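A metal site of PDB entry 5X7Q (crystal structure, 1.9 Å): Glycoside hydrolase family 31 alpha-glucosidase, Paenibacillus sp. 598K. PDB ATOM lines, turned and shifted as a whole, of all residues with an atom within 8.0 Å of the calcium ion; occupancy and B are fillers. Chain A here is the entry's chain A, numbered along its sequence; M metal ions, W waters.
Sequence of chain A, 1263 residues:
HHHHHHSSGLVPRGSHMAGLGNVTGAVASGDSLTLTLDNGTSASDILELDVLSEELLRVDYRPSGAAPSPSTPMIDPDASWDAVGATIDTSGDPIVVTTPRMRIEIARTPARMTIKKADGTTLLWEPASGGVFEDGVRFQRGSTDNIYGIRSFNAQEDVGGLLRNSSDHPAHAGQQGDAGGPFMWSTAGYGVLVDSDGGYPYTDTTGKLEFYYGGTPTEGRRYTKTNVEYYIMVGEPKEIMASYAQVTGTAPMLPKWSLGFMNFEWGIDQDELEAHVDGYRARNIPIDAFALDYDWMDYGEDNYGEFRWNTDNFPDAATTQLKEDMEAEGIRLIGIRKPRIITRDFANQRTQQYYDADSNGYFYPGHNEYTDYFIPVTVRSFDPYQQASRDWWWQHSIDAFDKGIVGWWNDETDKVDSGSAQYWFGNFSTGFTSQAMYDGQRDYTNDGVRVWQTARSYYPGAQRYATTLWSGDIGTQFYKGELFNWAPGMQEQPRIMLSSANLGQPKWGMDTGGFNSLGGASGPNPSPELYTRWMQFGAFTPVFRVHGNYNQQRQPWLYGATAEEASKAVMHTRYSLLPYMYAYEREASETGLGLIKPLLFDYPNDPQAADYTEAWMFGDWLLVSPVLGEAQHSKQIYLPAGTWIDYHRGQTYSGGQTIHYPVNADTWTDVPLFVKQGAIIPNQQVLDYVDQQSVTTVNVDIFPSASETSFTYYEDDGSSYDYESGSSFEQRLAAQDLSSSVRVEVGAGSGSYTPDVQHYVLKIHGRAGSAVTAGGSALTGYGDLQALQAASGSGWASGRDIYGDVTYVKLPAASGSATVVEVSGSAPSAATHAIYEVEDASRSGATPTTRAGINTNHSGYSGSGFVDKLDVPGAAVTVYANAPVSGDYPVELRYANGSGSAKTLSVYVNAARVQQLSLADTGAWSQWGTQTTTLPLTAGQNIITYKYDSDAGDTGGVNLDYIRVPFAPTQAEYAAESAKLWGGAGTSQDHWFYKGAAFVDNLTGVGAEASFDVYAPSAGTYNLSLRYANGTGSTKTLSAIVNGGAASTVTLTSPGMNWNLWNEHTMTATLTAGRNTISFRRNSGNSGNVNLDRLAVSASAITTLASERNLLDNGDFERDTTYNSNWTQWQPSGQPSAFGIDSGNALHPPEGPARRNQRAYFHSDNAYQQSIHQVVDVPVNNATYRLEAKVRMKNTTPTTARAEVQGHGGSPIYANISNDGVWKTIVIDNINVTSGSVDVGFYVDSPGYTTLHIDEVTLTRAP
The backbone carbonyl oxygen (O) of Asp 1093 sits at hydrogen-bond distance from the backbone NH (N) of Ala 976. The side-chain carboxylate of Asp 1093 is in salt-bridge range of the guanidinium group of Arg 1027, at 2.8 Å. NZ of Lys 995 lies within hydrogen-bond range of O of Glu 1108 (3.3 Å). The side-chain carboxylate (OE2) of Glu 977 sits close to the backbone NH (N) of Ala 997, at 3.4 Å.
Within 4 Å of the calcium ion: Glu 977, Lys 995, Ala 998 and Asp 1093.
The calcium ion is bound by water W1, the side-chain carboxylate (OD1) of Asp 1093, the backbone carbonyl oxygen (O) of Ala 998, the backbone carbonyl oxygen (O) of Lys 995, the side-chain carboxylate (OE1) of Glu 977 and the side-chain carboxylate (OE2) of Glu 977. Slightly farther from the calcium ion lies the backbone carbonyl oxygen (O) of Asp 1093 (3.0 Å).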
ATOM      1  N   HIS A 633       3.403  15.553 -22.025  1.00  0.00           N
ATOM      2  CA  HIS A 633       3.919  16.109 -20.751  1.00  0.00           C
ATOM      3  C   HIS A 633       3.112  15.749 -19.520  1.00  0.00           C
ATOM      4  O   HIS A 633       3.582  15.936 -18.394  1.00  0.00           O
ATOM      5  CB  HIS A 633       3.989  17.625 -20.835  1.00  0.00           C
ATOM      6  CG  HIS A 633       4.827  18.116 -21.973  1.00  0.00           C
ATOM      7  ND1 HIS A 633       6.203  18.069 -21.963  1.00  0.00           N
ATOM      8  CD2 HIS A 633       4.474  18.705 -23.143  1.00  0.00           C
ATOM      9  CE1 HIS A 633       6.669  18.605 -23.077  1.00  0.00           C
ATOM     10  NE2 HIS A 633       5.646  18.985 -23.818  1.00  0.00           N
ATOM     11  N   GLU A 973      11.752  20.011  -7.880  1.00  0.00           N
ATOM     12  CA  GLU A 973      11.383  20.779  -9.058  1.00  0.00           C
ATOM     13  C   GLU A 973      10.149  20.162  -9.707  1.00  0.00           C
ATOM     14  O   GLU A 973       9.932  18.965  -9.640  1.00  0.00           O
ATOM     15  CB  GLU A 973      12.537  20.859 -10.072  1.00  0.00           C
ATOM     16  CG  GLU A 973      12.991  19.517 -10.636  1.00  0.00           C
ATOM     17  CD  GLU A 973      14.078  19.693 -11.678  1.00  0.00           C
ATOM     18  OE1 GLU A 973      13.799  20.211 -12.786  1.00  0.00           O
ATOM     19  OE2 GLU A 973      15.234  19.329 -11.384  1.00  0.00           O
ATOM     20  N   TYR A 974       9.359  21.027 -10.331  1.00  0.00           N
ATOM     21  CA  TYR A 974       8.124  20.637 -10.994  1.00  0.00           C
ATOM     22  C   TYR A 974       8.118  21.386 -12.307  1.00  0.00           C
ATOM     23  O   TYR A 974       8.211  22.625 -12.314  1.00  0.00           O
ATOM     24  CB  TYR A 974       6.901  20.993 -10.117  1.00  0.00           C
ATOM     25  CG  TYR A 974       6.913  20.336  -8.748  1.00  0.00           C
ATOM     26  CD1 TYR A 974       7.590  20.911  -7.662  1.00  0.00           C
ATOM     27  CD2 TYR A 974       6.236  19.136  -8.534  1.00  0.00           C
ATOM     28  CE1 TYR A 974       7.609  20.302  -6.424  1.00  0.00           C
ATOM     29  CE2 TYR A 974       6.269  18.525  -7.298  1.00  0.00           C
ATOM     30  CZ  TYR A 974       6.944  19.104  -6.245  1.00  0.00           C
ATOM     31  OH  TYR A 974       6.929  18.467  -5.014  1.00  0.00           O
ATOM     32  N   ALA A 975       8.036  20.672 -13.413  1.00  0.00           N
ATOM     33  CA  ALA A 975       8.003  21.296 -14.727  1.00  0.00           C
ATOM     34  C   ALA A 975       6.636  21.947 -14.998  1.00  0.00           C
ATOM     35  O   ALA A 975       5.593  21.305 -14.860  1.00  0.00           O
ATOM     36  CB  ALA A 975       8.337  20.274 -15.798  1.00  0.00           C
ATOM     37  N   ALA A 976       6.663  23.203 -15.432  1.00  0.00           N
ATOM     38  CA  ALA A 976       5.442  23.909 -15.827  1.00  0.00           C
ATOM     39  C   ALA A 976       4.680  23.187 -16.940  1.00  0.00           C
ATOM     40  O   ALA A 976       3.455  23.044 -16.876  1.00  0.00           O
ATOM     41  CB  ALA A 976       5.789  25.326 -16.263  1.00  0.00           C
ATOM     42  N   GLU A 977       5.400  22.687 -17.928  1.00  0.00           N
ATOM     43  CA  GLU A 977       4.796  21.981 -19.071  1.00  0.00           C
ATOM     44  C   GLU A 977       4.028  20.703 -18.664  1.00  0.00           C
ATOM     45  O   GLU A 977       3.093  20.287 -19.365  1.00  0.00           O
ATOM     46  CB  GLU A 977       5.838  21.669 -20.144  1.00  0.00           C
ATOM     47  CG  GLU A 977       7.028  20.836 -19.665  1.00  0.00           C
ATOM     48  CD  GLU A 977       8.217  21.689 -19.235  1.00  0.00           C
ATOM     49  OE1 GLU A 977       8.021  22.807 -18.688  1.00  0.00           O
ATOM     50  OE2 GLU A 977       9.375  21.240 -19.453  1.00  0.00           O
ATOM     51  N   SER A 978       4.403  20.099 -17.535  1.00  0.00           N
ATOM     52  CA  SER A 978       3.705  18.929 -16.969  1.00  0.00           C
ATOM     53  C   SER A 978       2.632  19.250 -15.926  1.00  0.00           C
ATOM     54  O   SER A 978       1.963  18.327 -15.395  1.00  0.00           O
ATOM     55  CB  SER A 978       4.737  17.939 -16.388  1.00  0.00           C
ATOM     56  OG  SER A 978       5.616  17.479 -17.423  1.00  0.00           O
ATOM     57  N   SER A 988       4.963  25.044 -25.320  1.00  0.00           N
ATOM     58  CA  SER A 988       5.625  25.514 -26.519  1.00  0.00           C
ATOM     59  C   SER A 988       7.142  25.296 -26.428  1.00  0.00           C
ATOM     60  O   SER A 988       7.702  25.153 -25.326  1.00  0.00           O
ATOM     61  CB  SER A 988       5.331  26.992 -26.725  1.00  0.00           C
ATOM     62  OG  SER A 988       5.957  27.502 -27.908  1.00  0.00           O
ATOM     63  N   PHE A 993      16.213  28.642 -24.479  1.00  0.00           N
ATOM     64  CA  PHE A 993      16.744  28.597 -23.116  1.00  0.00           C
ATOM     65  C   PHE A 993      15.753  28.171 -22.026  1.00  0.00           C
ATOM     66  O   PHE A 993      16.003  28.385 -20.853  1.00  0.00           O
ATOM     67  CB  PHE A 993      17.469  29.911 -22.728  1.00  0.00           C
ATOM     68  CG  PHE A 993      18.716  30.164 -23.533  1.00  0.00           C
ATOM     69  CD1 PHE A 993      19.886  29.477 -23.241  1.00  0.00           C
ATOM     70  CD2 PHE A 993      18.700  31.047 -24.609  1.00  0.00           C
ATOM     71  CE1 PHE A 993      21.032  29.686 -23.986  1.00  0.00           C
ATOM     72  CE2 PHE A 993      19.849  31.272 -25.349  1.00  0.00           C
ATOM     73  CZ  PHE A 993      21.011  30.580 -25.054  1.00  0.00           C
ATOM     74  N   TYR A 994      14.665  27.520 -22.415  1.00  0.00           N
ATOM     75  CA  TYR A 994      13.817  26.812 -21.455  1.00  0.00           C
ATOM     76  C   TYR A 994      14.525  25.545 -20.932  1.00  0.00           C
ATOM     77  O   TYR A 994      15.435  25.008 -21.581  1.00  0.00           O
ATOM     78  CB  TYR A 994      12.462  26.423 -22.089  1.00  0.00           C
ATOM     79  CG  TYR A 994      12.542  25.557 -23.333  1.00  0.00           C
ATOM     80  CD1 TYR A 994      12.599  24.166 -23.253  1.00  0.00           C
ATOM     81  CD2 TYR A 994      12.514  26.128 -24.602  1.00  0.00           C
ATOM     82  CE1 TYR A 994      12.660  23.380 -24.392  1.00  0.00           C
ATOM     83  CE2 TYR A 994      12.576  25.355 -25.745  1.00  0.00           C
ATOM     84  CZ  TYR A 994      12.637  23.973 -25.635  1.00  0.00           C
ATOM     85  OH  TYR A 994      12.714  23.198 -26.780  1.00  0.00           O
ATOM     86  N   LYS A 995      14.081  25.101 -19.754  1.00  0.00           N
ATOM     87  CA  LYS A 995      14.526  23.846 -19.152  1.00  0.00           C
ATOM     88  C   LYS A 995      13.539  22.735 -19.475  1.00  0.00           C
ATOM     89  O   LYS A 995      12.351  22.993 -19.712  1.00  0.00           O
ATOM     90  CB  LYS A 995      14.652  23.997 -17.636  1.00  0.00           C
ATOM     91  CG  LYS A 995      15.536  25.137 -17.190  1.00  0.00           C
ATOM     92  CD  LYS A 995      16.979  24.955 -17.615  1.00  0.00           C
ATOM     93  CE  LYS A 995      17.811  26.142 -17.184  1.00  0.00           C
ATOM     94  NZ  LYS A 995      19.246  25.951 -17.542  1.00  0.00           N
ATOM     95  N   GLY A 996      14.026  21.508 -19.509  1.00  0.00           N
ATOM     96  CA  GLY A 996      13.191  20.362 -19.834  1.00  0.00           C
ATOM     97  C   GLY A 996      12.740  20.379 -21.275  1.00  0.00           C
ATOM     98  O   GLY A 996      13.391  21.001 -22.137  1.00  0.00           O
ATOM     99  N   ALA A 997      11.620  19.723 -21.552  1.00  0.00           N
ATOM    100  CA  ALA A 997      11.204  19.509 -22.931  1.00  0.00           C
ATOM    101  C   ALA A 997      10.425  20.696 -23.524  1.00  0.00           C
ATOM    102  O   ALA A 997      10.263  20.786 -24.736  1.00  0.00           O
ATOM    103  CB  ALA A 997      10.395  18.239 -23.045  1.00  0.00           C
ATOM    104  N   ALA A 998       9.948  21.594 -22.669  1.00  0.00           N
ATOM    105  CA  ALA A 998       9.126  22.721 -23.111  1.00  0.00           C
ATOM    106  C   ALA A 998       8.996  23.801 -22.037  1.00  0.00           C
ATOM    107  O   ALA A 998       9.677  23.753 -21.013  1.00  0.00           O
ATOM    108  CB  ALA A 998       7.739  22.215 -23.538  1.00  0.00           C
ATOM    109  N   PHE A 999       8.111  24.769 -22.297  1.00  0.00           N
ATOM    110  CA  PHE A 999       7.658  25.722 -21.304  1.00  0.00           C
ATOM    111  C   PHE A 999       6.166  26.002 -21.521  1.00  0.00           C
ATOM    112  O   PHE A 999       5.580  25.540 -22.517  1.00  0.00           O
ATOM    113  CB  PHE A 999       8.468  27.026 -21.368  1.00  0.00           C
ATOM    114  CG  PHE A 999       8.410  27.719 -22.688  1.00  0.00           C
ATOM    115  CD1 PHE A 999       7.420  28.667 -22.957  1.00  0.00           C
ATOM    116  CD2 PHE A 999       9.360  27.442 -23.661  1.00  0.00           C
ATOM    117  CE1 PHE A 999       7.353  29.290 -24.192  1.00  0.00           C
ATOM    118  CE2 PHE A 999       9.308  28.063 -24.898  1.00  0.00           C
ATOM    119  CZ  PHE A 999       8.307  28.989 -25.169  1.00  0.00           C
ATOM    120  N   VAL A1000       5.565  26.752 -20.593  1.00  0.00           N
ATOM    121  CA  VAL A1000       4.148  27.139 -20.675  1.00  0.00           C
ATOM    122  C   VAL A1000       4.000  28.586 -21.210  1.00  0.00           C
ATOM    123  O   VAL A1000       4.658  29.505 -20.728  1.00  0.00           O
ATOM    124  CB  VAL A1000       3.474  26.982 -19.312  1.00  0.00           C
ATOM    125  CG1 VAL A1000       2.084  27.611 -19.300  1.00  0.00           C
ATOM    126  CG2 VAL A1000       3.398  25.499 -18.931  1.00  0.00           C
ATOM    127  N   ARG A1027      10.580  29.930 -12.338  1.00  0.00           N
ATOM    128  CA  ARG A1027      11.338  30.391 -13.507  1.00  0.00           C
ATOM    129  C   ARG A1027      10.375  30.849 -14.596  1.00  0.00           C
ATOM    130  O   ARG A1027       9.484  30.094 -15.006  1.00  0.00           O
ATOM    131  CB  ARG A1027      12.226  29.268 -14.034  1.00  0.00           C
ATOM    132  CG  ARG A1027      13.205  29.700 -15.113  1.00  0.00           C
ATOM    133  CD  ARG A1027      14.180  28.554 -15.415  1.00  0.00           C
ATOM    134  NE  ARG A1027      15.378  29.017 -16.116  1.00  0.00           N
ATOM    135  CZ  ARG A1027      15.566  29.031 -17.435  1.00  0.00           C
ATOM    136  NH1 ARG A1027      14.648  28.612 -18.307  1.00  0.00           N
ATOM    137  NH2 ARG A1027      16.720  29.472 -17.912  1.00  0.00           N
ATOM    138  N   TRP A1062      15.305  34.297 -19.140  1.00  0.00           N
ATOM    139  CA  TRP A1062      14.508  33.697 -18.072  1.00  0.00           C
ATOM    140  C   TRP A1062      15.014  34.243 -16.741  1.00  0.00           C
ATOM    141  O   TRP A1062      16.198  34.519 -16.584  1.00  0.00           O
ATOM    142  CB  TRP A1062      14.613  32.177 -18.151  1.00  0.00           C
ATOM    143  CG  TRP A1062      14.065  31.616 -19.450  1.00  0.00           C
ATOM    144  CD1 TRP A1062      14.747  31.465 -20.629  1.00  0.00           C
ATOM    145  CD2 TRP A1062      12.736  31.161 -19.689  1.00  0.00           C
ATOM    146  NE1 TRP A1062      13.911  30.941 -21.588  1.00  0.00           N
ATOM    147  CE2 TRP A1062      12.673  30.741 -21.042  1.00  0.00           C
ATOM    148  CE3 TRP A1062      11.586  31.072 -18.894  1.00  0.00           C
ATOM    149  CZ2 TRP A1062      11.499  30.223 -21.614  1.00  0.00           C
ATOM    150  CZ3 TRP A1062      10.412  30.565 -19.480  1.00  0.00           C
ATOM    151  CH2 TRP A1062      10.385  30.138 -20.815  1.00  0.00           C
ATOM    152  N   LEU A1092       5.980  30.480 -18.290  1.00  0.00           N
ATOM    153  CA  LEU A1092       6.443  29.791 -17.087  1.00  0.00           C
ATOM    154  C   LEU A1092       7.177  28.494 -17.466  1.00  0.00           C
ATOM    155  O   LEU A1092       6.756  27.791 -18.385  1.00  0.00           O
ATOM    156  CB  LEU A1092       5.270  29.464 -16.156  1.00  0.00           C
ATOM    157  CG  LEU A1092       4.352  30.631 -15.763  1.00  0.00           C
ATOM    158  CD1 LEU A1092       3.264  30.114 -14.832  1.00  0.00           C
ATOM    159  CD2 LEU A1092       5.107  31.781 -15.121  1.00  0.00           C
ATOM    160  N   ASP A1093       8.245  28.186 -16.742  1.00  0.00           N
ATOM    161  CA  ASP A1093       9.093  27.049 -17.090  1.00  0.00           C
ATOM    162  C   ASP A1093       9.162  25.962 -16.026  1.00  0.00           C
ATOM    163  O   ASP A1093       9.106  24.774 -16.345  1.00  0.00           O
ATOM    164  CB  ASP A1093      10.487  27.565 -17.395  1.00  0.00           C
ATOM    165  CG  ASP A1093      11.334  26.595 -18.192  1.00  0.00           C
ATOM    166  OD1 ASP A1093      10.796  25.648 -18.790  1.00  0.00           O
ATOM    167  OD2 ASP A1093      12.564  26.797 -18.232  1.00  0.00           O
ATOM    168  N   ARG A1094       9.307  26.366 -14.765  1.00  0.00           N
ATOM    169  CA  ARG A1094       9.611  25.429 -13.676  1.00  0.00           C
ATOM    170  C   ARG A1094       9.356  26.062 -12.315  1.00  0.00           C
ATOM    171  O   ARG A1094       9.680  27.238 -12.097  1.00  0.00           O
ATOM    172  CB  ARG A1094      11.091  24.971 -13.773  1.00  0.00           C
ATOM    173  CG  ARG A1094      11.532  23.970 -12.718  1.00  0.00           C
ATOM    174  CD  ARG A1094      12.207  24.628 -11.509  1.00  0.00           C
ATOM    175  NE  ARG A1094      13.408  25.359 -11.920  1.00  0.00           N
ATOM    176  CZ  ARG A1094      13.688  26.638 -11.652  1.00  0.00           C
ATOM    177  NH1 ARG A1094      12.889  27.415 -10.932  1.00  0.00           N
ATOM    178  NH2 ARG A1094      14.835  27.143 -12.094  1.00  0.00           N
ATOM    179  N   LEU A1095       8.800  25.279 -11.410  1.00  0.00           N
ATOM    180  CA  LEU A1095       8.681  25.641 -10.001  1.00  0.00           C
ATOM    181  C   LEU A1095       9.652  24.816  -9.154  1.00  0.00           C
ATOM    182  O   LEU A1095       9.562  23.593  -9.141  1.00  0.00           O
ATOM    183  CB  LEU A1095       7.257  25.402  -9.510  1.00  0.00           C
ATOM    184  CG  LEU A1095       6.961  25.861  -8.080  1.00  0.00           C
ATOM    185  CD1 LEU A1095       7.070  27.368  -7.937  1.00  0.00           C
ATOM    186  CD2 LEU A1095       5.566  25.371  -7.689  1.00  0.00           C
ATOM    187  N   GLU A1108      19.766  21.692 -14.201  1.00  0.00           N
ATOM    188  CA  GLU A1108      19.744  22.966 -14.906  1.00  0.00           C
ATOM    189  C   GLU A1108      21.130  23.593 -15.052  1.00  0.00           C
ATOM    190  O   GLU A1108      21.241  24.792 -15.230  1.00  0.00           O
ATOM    191  CB  GLU A1108      18.790  23.943 -14.179  1.00  0.00           C
ATOM    192  CG  GLU A1108      17.352  23.424 -14.140  1.00  0.00           C
ATOM    193  CD  GLU A1108      16.352  24.444 -13.629  1.00  0.00           C
ATOM    194  OE1 GLU A1108      16.743  25.562 -13.236  1.00  0.00           O
ATOM    195  OE2 GLU A1108      15.126  24.122 -13.639  1.00  0.00           O
HETATM  196 CA    CA M   1      10.304  23.560 -18.842  1.00  0.00          CA
HETATM  197  O   HOH W   1      10.936  22.876 -17.025  1.00  0.00           O
